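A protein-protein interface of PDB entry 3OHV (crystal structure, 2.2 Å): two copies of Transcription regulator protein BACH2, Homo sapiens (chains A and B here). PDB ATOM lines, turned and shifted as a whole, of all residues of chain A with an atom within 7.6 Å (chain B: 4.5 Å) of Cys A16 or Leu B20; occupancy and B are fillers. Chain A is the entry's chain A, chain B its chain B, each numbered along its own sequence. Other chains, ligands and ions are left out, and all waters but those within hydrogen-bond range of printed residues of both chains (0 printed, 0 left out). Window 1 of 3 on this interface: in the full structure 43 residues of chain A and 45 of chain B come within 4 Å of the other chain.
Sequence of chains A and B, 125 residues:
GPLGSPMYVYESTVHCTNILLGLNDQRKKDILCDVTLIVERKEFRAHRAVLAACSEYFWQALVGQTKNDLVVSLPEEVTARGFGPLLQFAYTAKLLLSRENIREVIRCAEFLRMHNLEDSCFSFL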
ATOM      1  N   SER A  12     -17.319   6.751 -11.311  1.00  0.00           N
ATOM      2  CA  SER A  12     -16.890   6.798  -9.914  1.00  0.00           C
ATOM      3  C   SER A  12     -15.644   7.665  -9.803  1.00  0.00           C
ATOM      4  O   SER A  12     -14.679   7.473 -10.546  1.00  0.00           O
ATOM      5  CB  SER A  12     -16.645   5.387  -9.368  1.00  0.00           C
ATOM      6  OG  SER A  12     -16.237   5.432  -8.013  1.00  0.00           O
ATOM      7  N   THR A  13     -15.697   8.645  -8.906  1.00  0.00           N
ATOM      8  CA  THR A  13     -14.598   9.596  -8.692  1.00  0.00           C
ATOM      9  C   THR A  13     -13.637   9.119  -7.606  1.00  0.00           C
ATOM     10  O   THR A  13     -12.580   9.712  -7.398  1.00  0.00           O
ATOM     11  CB  THR A  13     -15.112  11.027  -8.347  1.00  0.00           C
ATOM     12  OG1 THR A  13     -15.907  10.981  -7.150  1.00  0.00           O
ATOM     13  CG2 THR A  13     -15.945  11.607  -9.510  1.00  0.00           C
ATOM     14  N   VAL A  14     -14.018   8.044  -6.923  1.00  0.00           N
ATOM     15  CA  VAL A  14     -13.150   7.376  -5.975  1.00  0.00           C
ATOM     16  C   VAL A  14     -12.512   6.093  -6.541  1.00  0.00           C
ATOM     17  O   VAL A  14     -11.500   5.629  -6.004  1.00  0.00           O
ATOM     18  CB  VAL A  14     -13.893   7.017  -4.662  1.00  0.00           C
ATOM     19  CG1 VAL A  14     -14.286   8.274  -3.895  1.00  0.00           C
ATOM     20  CG2 VAL A  14     -15.103   6.147  -4.947  1.00  0.00           C
ATOM     21  N   HIS A  15     -13.090   5.527  -7.608  1.00  0.00           N
ATOM     22  CA  HIS A  15     -12.678   4.194  -8.040  1.00  0.00           C
ATOM     23  C   HIS A  15     -11.167   4.022  -8.255  1.00  0.00           C
ATOM     24  O   HIS A  15     -10.564   3.136  -7.652  1.00  0.00           O
ATOM     25  CB  HIS A  15     -13.465   3.673  -9.242  1.00  0.00           C
ATOM     26  CG  HIS A  15     -13.033   2.309  -9.684  1.00  0.00           C
ATOM     27  ND1 HIS A  15     -13.468   1.155  -9.069  1.00  0.00           N
ATOM     28  CD2 HIS A  15     -12.173   1.919 -10.656  1.00  0.00           C
ATOM     29  CE1 HIS A  15     -12.905   0.111  -9.653  1.00  0.00           C
ATOM     30  NE2 HIS A  15     -12.118   0.547 -10.622  1.00  0.00           N
ATOM     31  N   CYS A  16     -10.571   4.878  -9.079  1.00  0.00           N
ATOM     32  CA  CYS A  16      -9.143   4.795  -9.359  1.00  0.00           C
ATOM     33  C   CYS A  16      -8.269   4.826  -8.093  1.00  0.00           C
ATOM     34  O   CYS A  16      -7.517   3.887  -7.817  1.00  0.00           O
ATOM     35  CB  CYS A  16      -8.714   5.878 -10.328  1.00  0.00           C
ATOM     36  SG  CYS A  16      -7.139   5.445 -11.092  1.00  0.00           S
ATOM     37  N   THR A  17      -8.392   5.899  -7.324  1.00  0.00           N
ATOM     38  CA  THR A  17      -7.762   6.014  -6.027  1.00  0.00           C
ATOM     39  C   THR A  17      -7.903   4.743  -5.218  1.00  0.00           C
ATOM     40  O   THR A  17      -6.932   4.298  -4.593  1.00  0.00           O
ATOM     41  CB  THR A  17      -8.360   7.200  -5.235  1.00  0.00           C
ATOM     42  OG1 THR A  17      -7.910   8.408  -5.834  1.00  0.00           O
ATOM     43  CG2 THR A  17      -7.947   7.194  -3.733  1.00  0.00           C
ATOM     44  N   ASN A  18      -9.109   4.189  -5.190  1.00  0.00           N
ATOM     45  CA  ASN A  18      -9.384   2.972  -4.422  1.00  0.00           C
ATOM     46  C   ASN A  18      -8.564   1.792  -4.953  1.00  0.00           C
ATOM     47  O   ASN A  18      -8.004   1.035  -4.173  1.00  0.00           O
ATOM     48  CB  ASN A  18     -10.902   2.647  -4.401  1.00  0.00           C
ATOM     49  CG  ASN A  18     -11.692   3.500  -3.379  1.00  0.00           C
ATOM     50  OD1 ASN A  18     -11.160   3.894  -2.321  1.00  0.00           O
ATOM     51  ND2 ASN A  18     -12.977   3.752  -3.680  1.00  0.00           N
ATOM     52  N   ILE A  19      -8.485   1.653  -6.281  1.00  0.00           N
ATOM     53  CA  ILE A  19      -7.702   0.580  -6.892  1.00  0.00           C
ATOM     54  C   ILE A  19      -6.234   0.741  -6.533  1.00  0.00           C
ATOM     55  O   ILE A  19      -5.567  -0.222  -6.138  1.00  0.00           O
ATOM     56  CB  ILE A  19      -7.840   0.551  -8.448  1.00  0.00           C
ATOM     57  CG1 ILE A  19      -9.278   0.219  -8.876  1.00  0.00           C
ATOM     58  CG2 ILE A  19      -6.824  -0.428  -9.067  1.00  0.00           C
ATOM     59  CD1 ILE A  19      -9.849  -1.118  -8.342  1.00  0.00           C
ATOM     60  N   LEU A  20      -5.737   1.972  -6.665  1.00  0.00           N
ATOM     61  CA  LEU A  20      -4.337   2.234  -6.413  1.00  0.00           C
ATOM     62  C   LEU A  20      -3.991   1.978  -4.921  1.00  0.00           C
ATOM     63  O   LEU A  20      -2.960   1.382  -4.618  1.00  0.00           O
ATOM     64  CB  LEU A  20      -3.961   3.642  -6.919  1.00  0.00           C
ATOM     65  CG  LEU A  20      -2.517   3.947  -7.349  1.00  0.00           C
ATOM     66  CD1 LEU A  20      -1.921   2.951  -8.371  1.00  0.00           C
ATOM     67  CD2 LEU A  20      -2.408   5.366  -7.915  1.00  0.00           C
ATOM     68  N   LEU A  21      -4.859   2.387  -3.995  1.00  0.00           N
ATOM     69  CA  LEU A  21      -4.656   2.048  -2.564  1.00  0.00           C
ATOM     70  C   LEU A  21      -4.612   0.514  -2.337  1.00  0.00           C
ATOM     71  O   LEU A  21      -3.836   0.037  -1.513  1.00  0.00           O
ATOM     72  CB  LEU A  21      -5.765   2.630  -1.693  1.00  0.00           C
ATOM     73  CG  LEU A  21      -5.758   4.067  -1.135  1.00  0.00           C
ATOM     74  CD1 LEU A  21      -7.180   4.448  -0.578  1.00  0.00           C
ATOM     75  CD2 LEU A  21      -4.661   4.279  -0.061  1.00  0.00           C
ATOM     76  N   GLY A  22      -5.438  -0.241  -3.073  1.00  0.00           N
ATOM     77  CA  GLY A  22      -5.533  -1.684  -2.908  1.00  0.00           C
ATOM     78  C   GLY A  22      -4.242  -2.321  -3.403  1.00  0.00           C
ATOM     79  O   GLY A  22      -3.705  -3.237  -2.772  1.00  0.00           O
ATOM     80  N   LEU A  23      -3.762  -1.822  -4.547  1.00  0.00           N
ATOM     81  CA  LEU A  23      -2.472  -2.191  -5.111  1.00  0.00           C
ATOM     82  C   LEU A  23      -1.264  -1.853  -4.208  1.00  0.00           C
ATOM     83  O   LEU A  23      -0.371  -2.679  -4.025  1.00  0.00           O
ATOM     84  CB  LEU A  23      -2.303  -1.514  -6.468  1.00  0.00           C
ATOM     85  CG  LEU A  23      -3.234  -2.015  -7.584  1.00  0.00           C
ATOM     86  CD1 LEU A  23      -2.953  -1.238  -8.843  1.00  0.00           C
ATOM     87  CD2 LEU A  23      -3.151  -3.514  -7.849  1.00  0.00           C
ATOM     88  N   ALA A  53       3.067   0.130 -16.735  1.00  0.00           N
ATOM     89  CA  ALA A  53       2.143   1.211 -17.071  1.00  0.00           C
ATOM     90  C   ALA A  53       2.678   2.600 -16.708  1.00  0.00           C
ATOM     91  O   ALA A  53       2.299   3.589 -17.326  1.00  0.00           O
ATOM     92  CB  ALA A  53       0.744   0.945 -16.485  1.00  0.00           C
ATOM     93  N   CYS B  16      -3.116   8.257 -11.487  1.00  0.00           N
ATOM     94  CA  CYS B  16      -4.031   7.131 -11.320  1.00  0.00           C
ATOM     95  C   CYS B  16      -4.784   6.806 -12.610  1.00  0.00           C
ATOM     96  O   CYS B  16      -4.870   5.655 -12.997  1.00  0.00           O
ATOM     97  CB  CYS B  16      -5.022   7.380 -10.191  1.00  0.00           C
ATOM     98  SG  CYS B  16      -5.775   5.843  -9.617  1.00  0.00           S
ATOM     99  N   THR B  17      -5.332   7.819 -13.268  1.00  0.00           N
ATOM    100  CA  THR B  17      -6.136   7.590 -14.462  1.00  0.00           C
ATOM    101  C   THR B  17      -5.270   7.039 -15.595  1.00  0.00           C
ATOM    102  O   THR B  17      -5.678   6.115 -16.269  1.00  0.00           O
ATOM    103  CB  THR B  17      -6.890   8.868 -14.925  1.00  0.00           C
ATOM    104  OG1 THR B  17      -6.075  10.007 -14.660  1.00  0.00           O
ATOM    105  CG2 THR B  17      -8.187   9.051 -14.164  1.00  0.00           C
ATOM    106  N   ASN B  18      -4.083   7.612 -15.787  1.00  0.00           N
ATOM    107  CA  ASN B  18      -3.103   7.090 -16.737  1.00  0.00           C
ATOM    108  C   ASN B  18      -2.607   5.659 -16.487  1.00  0.00           C
ATOM    109  O   ASN B  18      -2.326   4.933 -17.446  1.00  0.00           O
ATOM    110  CB  ASN B  18      -1.894   8.014 -16.829  1.00  0.00           C
ATOM    111  CG  ASN B  18      -2.199   9.315 -17.560  1.00  0.00           C
ATOM    112  OD1 ASN B  18      -3.237   9.462 -18.221  1.00  0.00           O
ATOM    113  ND2 ASN B  18      -1.279  10.271 -17.443  1.00  0.00           N
ATOM    114  N   ILE B  19      -2.484   5.274 -15.216  1.00  0.00           N
ATOM    115  CA  ILE B  19      -2.093   3.924 -14.827  1.00  0.00           C
ATOM    116  C   ILE B  19      -3.183   2.949 -15.252  1.00  0.00           C
ATOM    117  O   ILE B  19      -2.913   1.872 -15.791  1.00  0.00           O
ATOM    118  CB  ILE B  19      -1.851   3.852 -13.285  1.00  0.00           C
ATOM    119  CG1 ILE B  19      -0.547   4.550 -12.948  1.00  0.00           C
ATOM    120  CG2 ILE B  19      -1.857   2.422 -12.740  1.00  0.00           C
ATOM    121  CD1 ILE B  19       0.659   4.048 -13.784  1.00  0.00           C
ATOM    122  N   LEU B  20      -4.419   3.370 -15.022  1.00  0.00           N
ATOM    123  CA  LEU B  20      -5.596   2.574 -15.266  1.00  0.00           C
ATOM    124  C   LEU B  20      -5.855   2.407 -16.749  1.00  0.00           C
ATOM    125  O   LEU B  20      -6.219   1.321 -17.194  1.00  0.00           O
ATOM    126  CB  LEU B  20      -6.788   3.254 -14.598  1.00  0.00           C
ATOM    127  CG  LEU B  20      -7.720   2.304 -13.880  1.00  0.00           C
ATOM    128  CD1 LEU B  20      -6.995   1.443 -12.831  1.00  0.00           C
ATOM    129  CD2 LEU B  20      -8.833   3.103 -13.268  1.00  0.00           C
ATOM    130  N   LEU B  21      -5.666   3.483 -17.504  1.00  0.00           N
ATOM    131  CA  LEU B  21      -5.697   3.458 -18.959  1.00  0.00           C
ATOM    132  C   LEU B  21      -4.648   2.477 -19.516  1.00  0.00           C
ATOM    133  O   LEU B  21      -4.877   1.806 -20.529  1.00  0.00           O
ATOM    134  CB  LEU B  21      -5.410   4.870 -19.500  1.00  0.00           C
ATOM    135  CG  LEU B  21      -6.464   5.993 -19.555  1.00  0.00           C
ATOM    136  CD1 LEU B  21      -5.771   7.317 -19.813  1.00  0.00           C
ATOM    137  CD2 LEU B  21      -7.533   5.753 -20.632  1.00  0.00           C
ATOM    138  N   GLY B  22      -3.495   2.413 -18.843  1.00  0.00           N
ATOM    139  CA  GLY B  22      -2.383   1.564 -19.261  1.00  0.00           C
ATOM    140  C   GLY B  22      -2.743   0.115 -19.026  1.00  0.00           C
ATOM    141  O   GLY B  22      -2.539  -0.741 -19.896  1.00  0.00           O
ATOM    142  N   LEU B  23      -3.314  -0.151 -17.859  1.00  0.00           N
ATOM    143  CA  LEU B  23      -3.720  -1.495 -17.494  1.00  0.00           C
ATOM    144  C   LEU B  23      -4.879  -1.999 -18.361  1.00  0.00           C
ATOM    145  O   LEU B  23      -4.911  -3.165 -18.747  1.00  0.00           O
ATOM    146  CB  LEU B  23      -4.060  -1.574 -16.002  1.00  0.00           C
ATOM    147  CG  LEU B  23      -2.912  -1.328 -15.012  1.00  0.00           C
ATOM    148  CD1 LEU B  23      -3.409  -1.227 -13.535  1.00  0.00           C
ATOM    149  CD2 LEU B  23      -1.777  -2.372 -15.128  1.00  0.00           C
ATOM    150  N   ASN B  24      -5.839  -1.129 -18.654  1.00  0.00           N
ATOM    151  CA  ASN B  24      -6.959  -1.494 -19.539  1.00  0.00           C
ATOM    152  C   ASN B  24      -6.469  -1.813 -20.951  1.00  0.00           C
ATOM    153  O   ASN B  24      -6.881  -2.806 -21.540  1.00  0.00           O
ATOM    154  CB  ASN B  24      -8.021  -0.385 -19.583  1.00  0.00           C
ATOM    155  CG  ASN B  24      -9.365  -0.876 -20.108  1.00  0.00           C
ATOM    156  OD1 ASN B  24      -9.871  -1.926 -19.701  1.00  0.00           O
ATOM    157  ND2 ASN B  24      -9.950  -0.114 -21.005  1.00  0.00           N
ATOM    158  N   TYR B  91     -11.652  -1.427 -14.770  1.00  0.00           N
ATOM    159  CA  TYR B  91     -10.484  -0.866 -15.464  1.00  0.00           C
ATOM    160  C   TYR B  91     -10.633   0.580 -15.943  1.00  0.00           C
ATOM    161  O   TYR B  91      -9.674   1.142 -16.508  1.00  0.00           O
ATOM    162  CB  TYR B  91     -10.081  -1.737 -16.658  1.00  0.00           C
ATOM    163  CG  TYR B  91      -9.315  -2.987 -16.302  1.00  0.00           C
ATOM    164  CD1 TYR B  91      -7.922  -3.014 -16.383  1.00  0.00           C
ATOM    165  CD2 TYR B  91      -9.976  -4.133 -15.919  1.00  0.00           C
ATOM    166  CE1 TYR B  91      -7.209  -4.137 -16.075  1.00  0.00           C
ATOM    167  CE2 TYR B  91      -9.277  -5.277 -15.595  1.00  0.00           C
ATOM    168  CZ  TYR B  91      -7.889  -5.275 -15.678  1.00  0.00           C
ATOM    169  OH  TYR B  91      -7.188  -6.399 -15.364  1.00  0.00           O
ATOM    170  N   THR B  92     -11.816   1.172 -15.747  1.00  0.00           N
ATOM    171  CA  THR B  92     -12.100   2.522 -16.251  1.00  0.00           C
ATOM    172  C   THR B  92     -12.746   3.476 -15.255  1.00  0.00           C
ATOM    173  O   THR B  92     -12.720   4.694 -15.466  1.00  0.00           O
ATOM    174  CB  THR B  92     -12.997   2.490 -17.490  1.00  0.00           C
ATOM    175  OG1 THR B  92     -14.197   1.748 -17.192  1.00  0.00           O
ATOM    176  CG2 THR B  92     -12.238   1.876 -18.690  1.00  0.00           C
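Among the printed residues, pairs that only touch across the chains: Cys A16 with Leu B20 (3.6 Å), Leu A20 with Cys B16 (3.8 Å) and Ala A53 with Ile B19 (3.8 Å).
Cys A16 touches its own counterpart, Cys B16.
Cys A16 touches Thr B17, and with the chains exchanged Thr A17 touches Cys B16.
Cys A16 touches Leu B20, and with the chains exchanged Leu A20 touches Cys B16.
8 positions are printed for both chains.
Of the 6 pairs that touch across the chains among the printed residues, 5 have their exchanged pair printed and touching as well.
The side-chain sulfur of Cys A16 is disulfide-bonded to the side-chain sulfur of Cys B16, at 2.0 Å.
SG of Cys A16 sits at hydrogen-bond distance from N of Thr B17 (3.7 Å).
The backbone NH (N) of Thr A17 is in hydrogen-bond range of the side-chain sulfur (SG) of Cys B16 (3.5 Å).
Thr A13 touches none of the printed residues of chain B.
Cys A16 touches just these residues of chain B: Cys B16, Thr B17 and Leu B20.
Printed residues of chain B within 4 Å of Thr A17: Cys B16.
Of the printed residues of chain B, Leu A20 touches Cys B16.
Of the printed residues of chain A, Thr B17 touches Cys A16.
Of the printed residues of chain A, Ile B19 touches Ala A53.
Leu B20 touches just one residue of chain A: Cys A16.
The nearest printed residue of chain B that does not touch Cys A16 is Ile B19 (5.9 Å).
The nearest residue of chain A that does not touch Leu B20 is Ile A19 (4.2 Å).
Printed residues of chain B that touch a printed residue of chain A: Cys B16, Thr B17, Ile B19 and Leu B20.
Of the 13 printed residues of chain A, 4 touch a printed residue of chain B.
Printed residues of chain A that touch a printed residue of chain B: Cys A16, Thr A17, Leu A20 and Ala A53.
Among the printed residues, no Asp or Glu carboxylate lies within 4 Å of a Lys or Arg side-chain nitrogen of the other chain.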
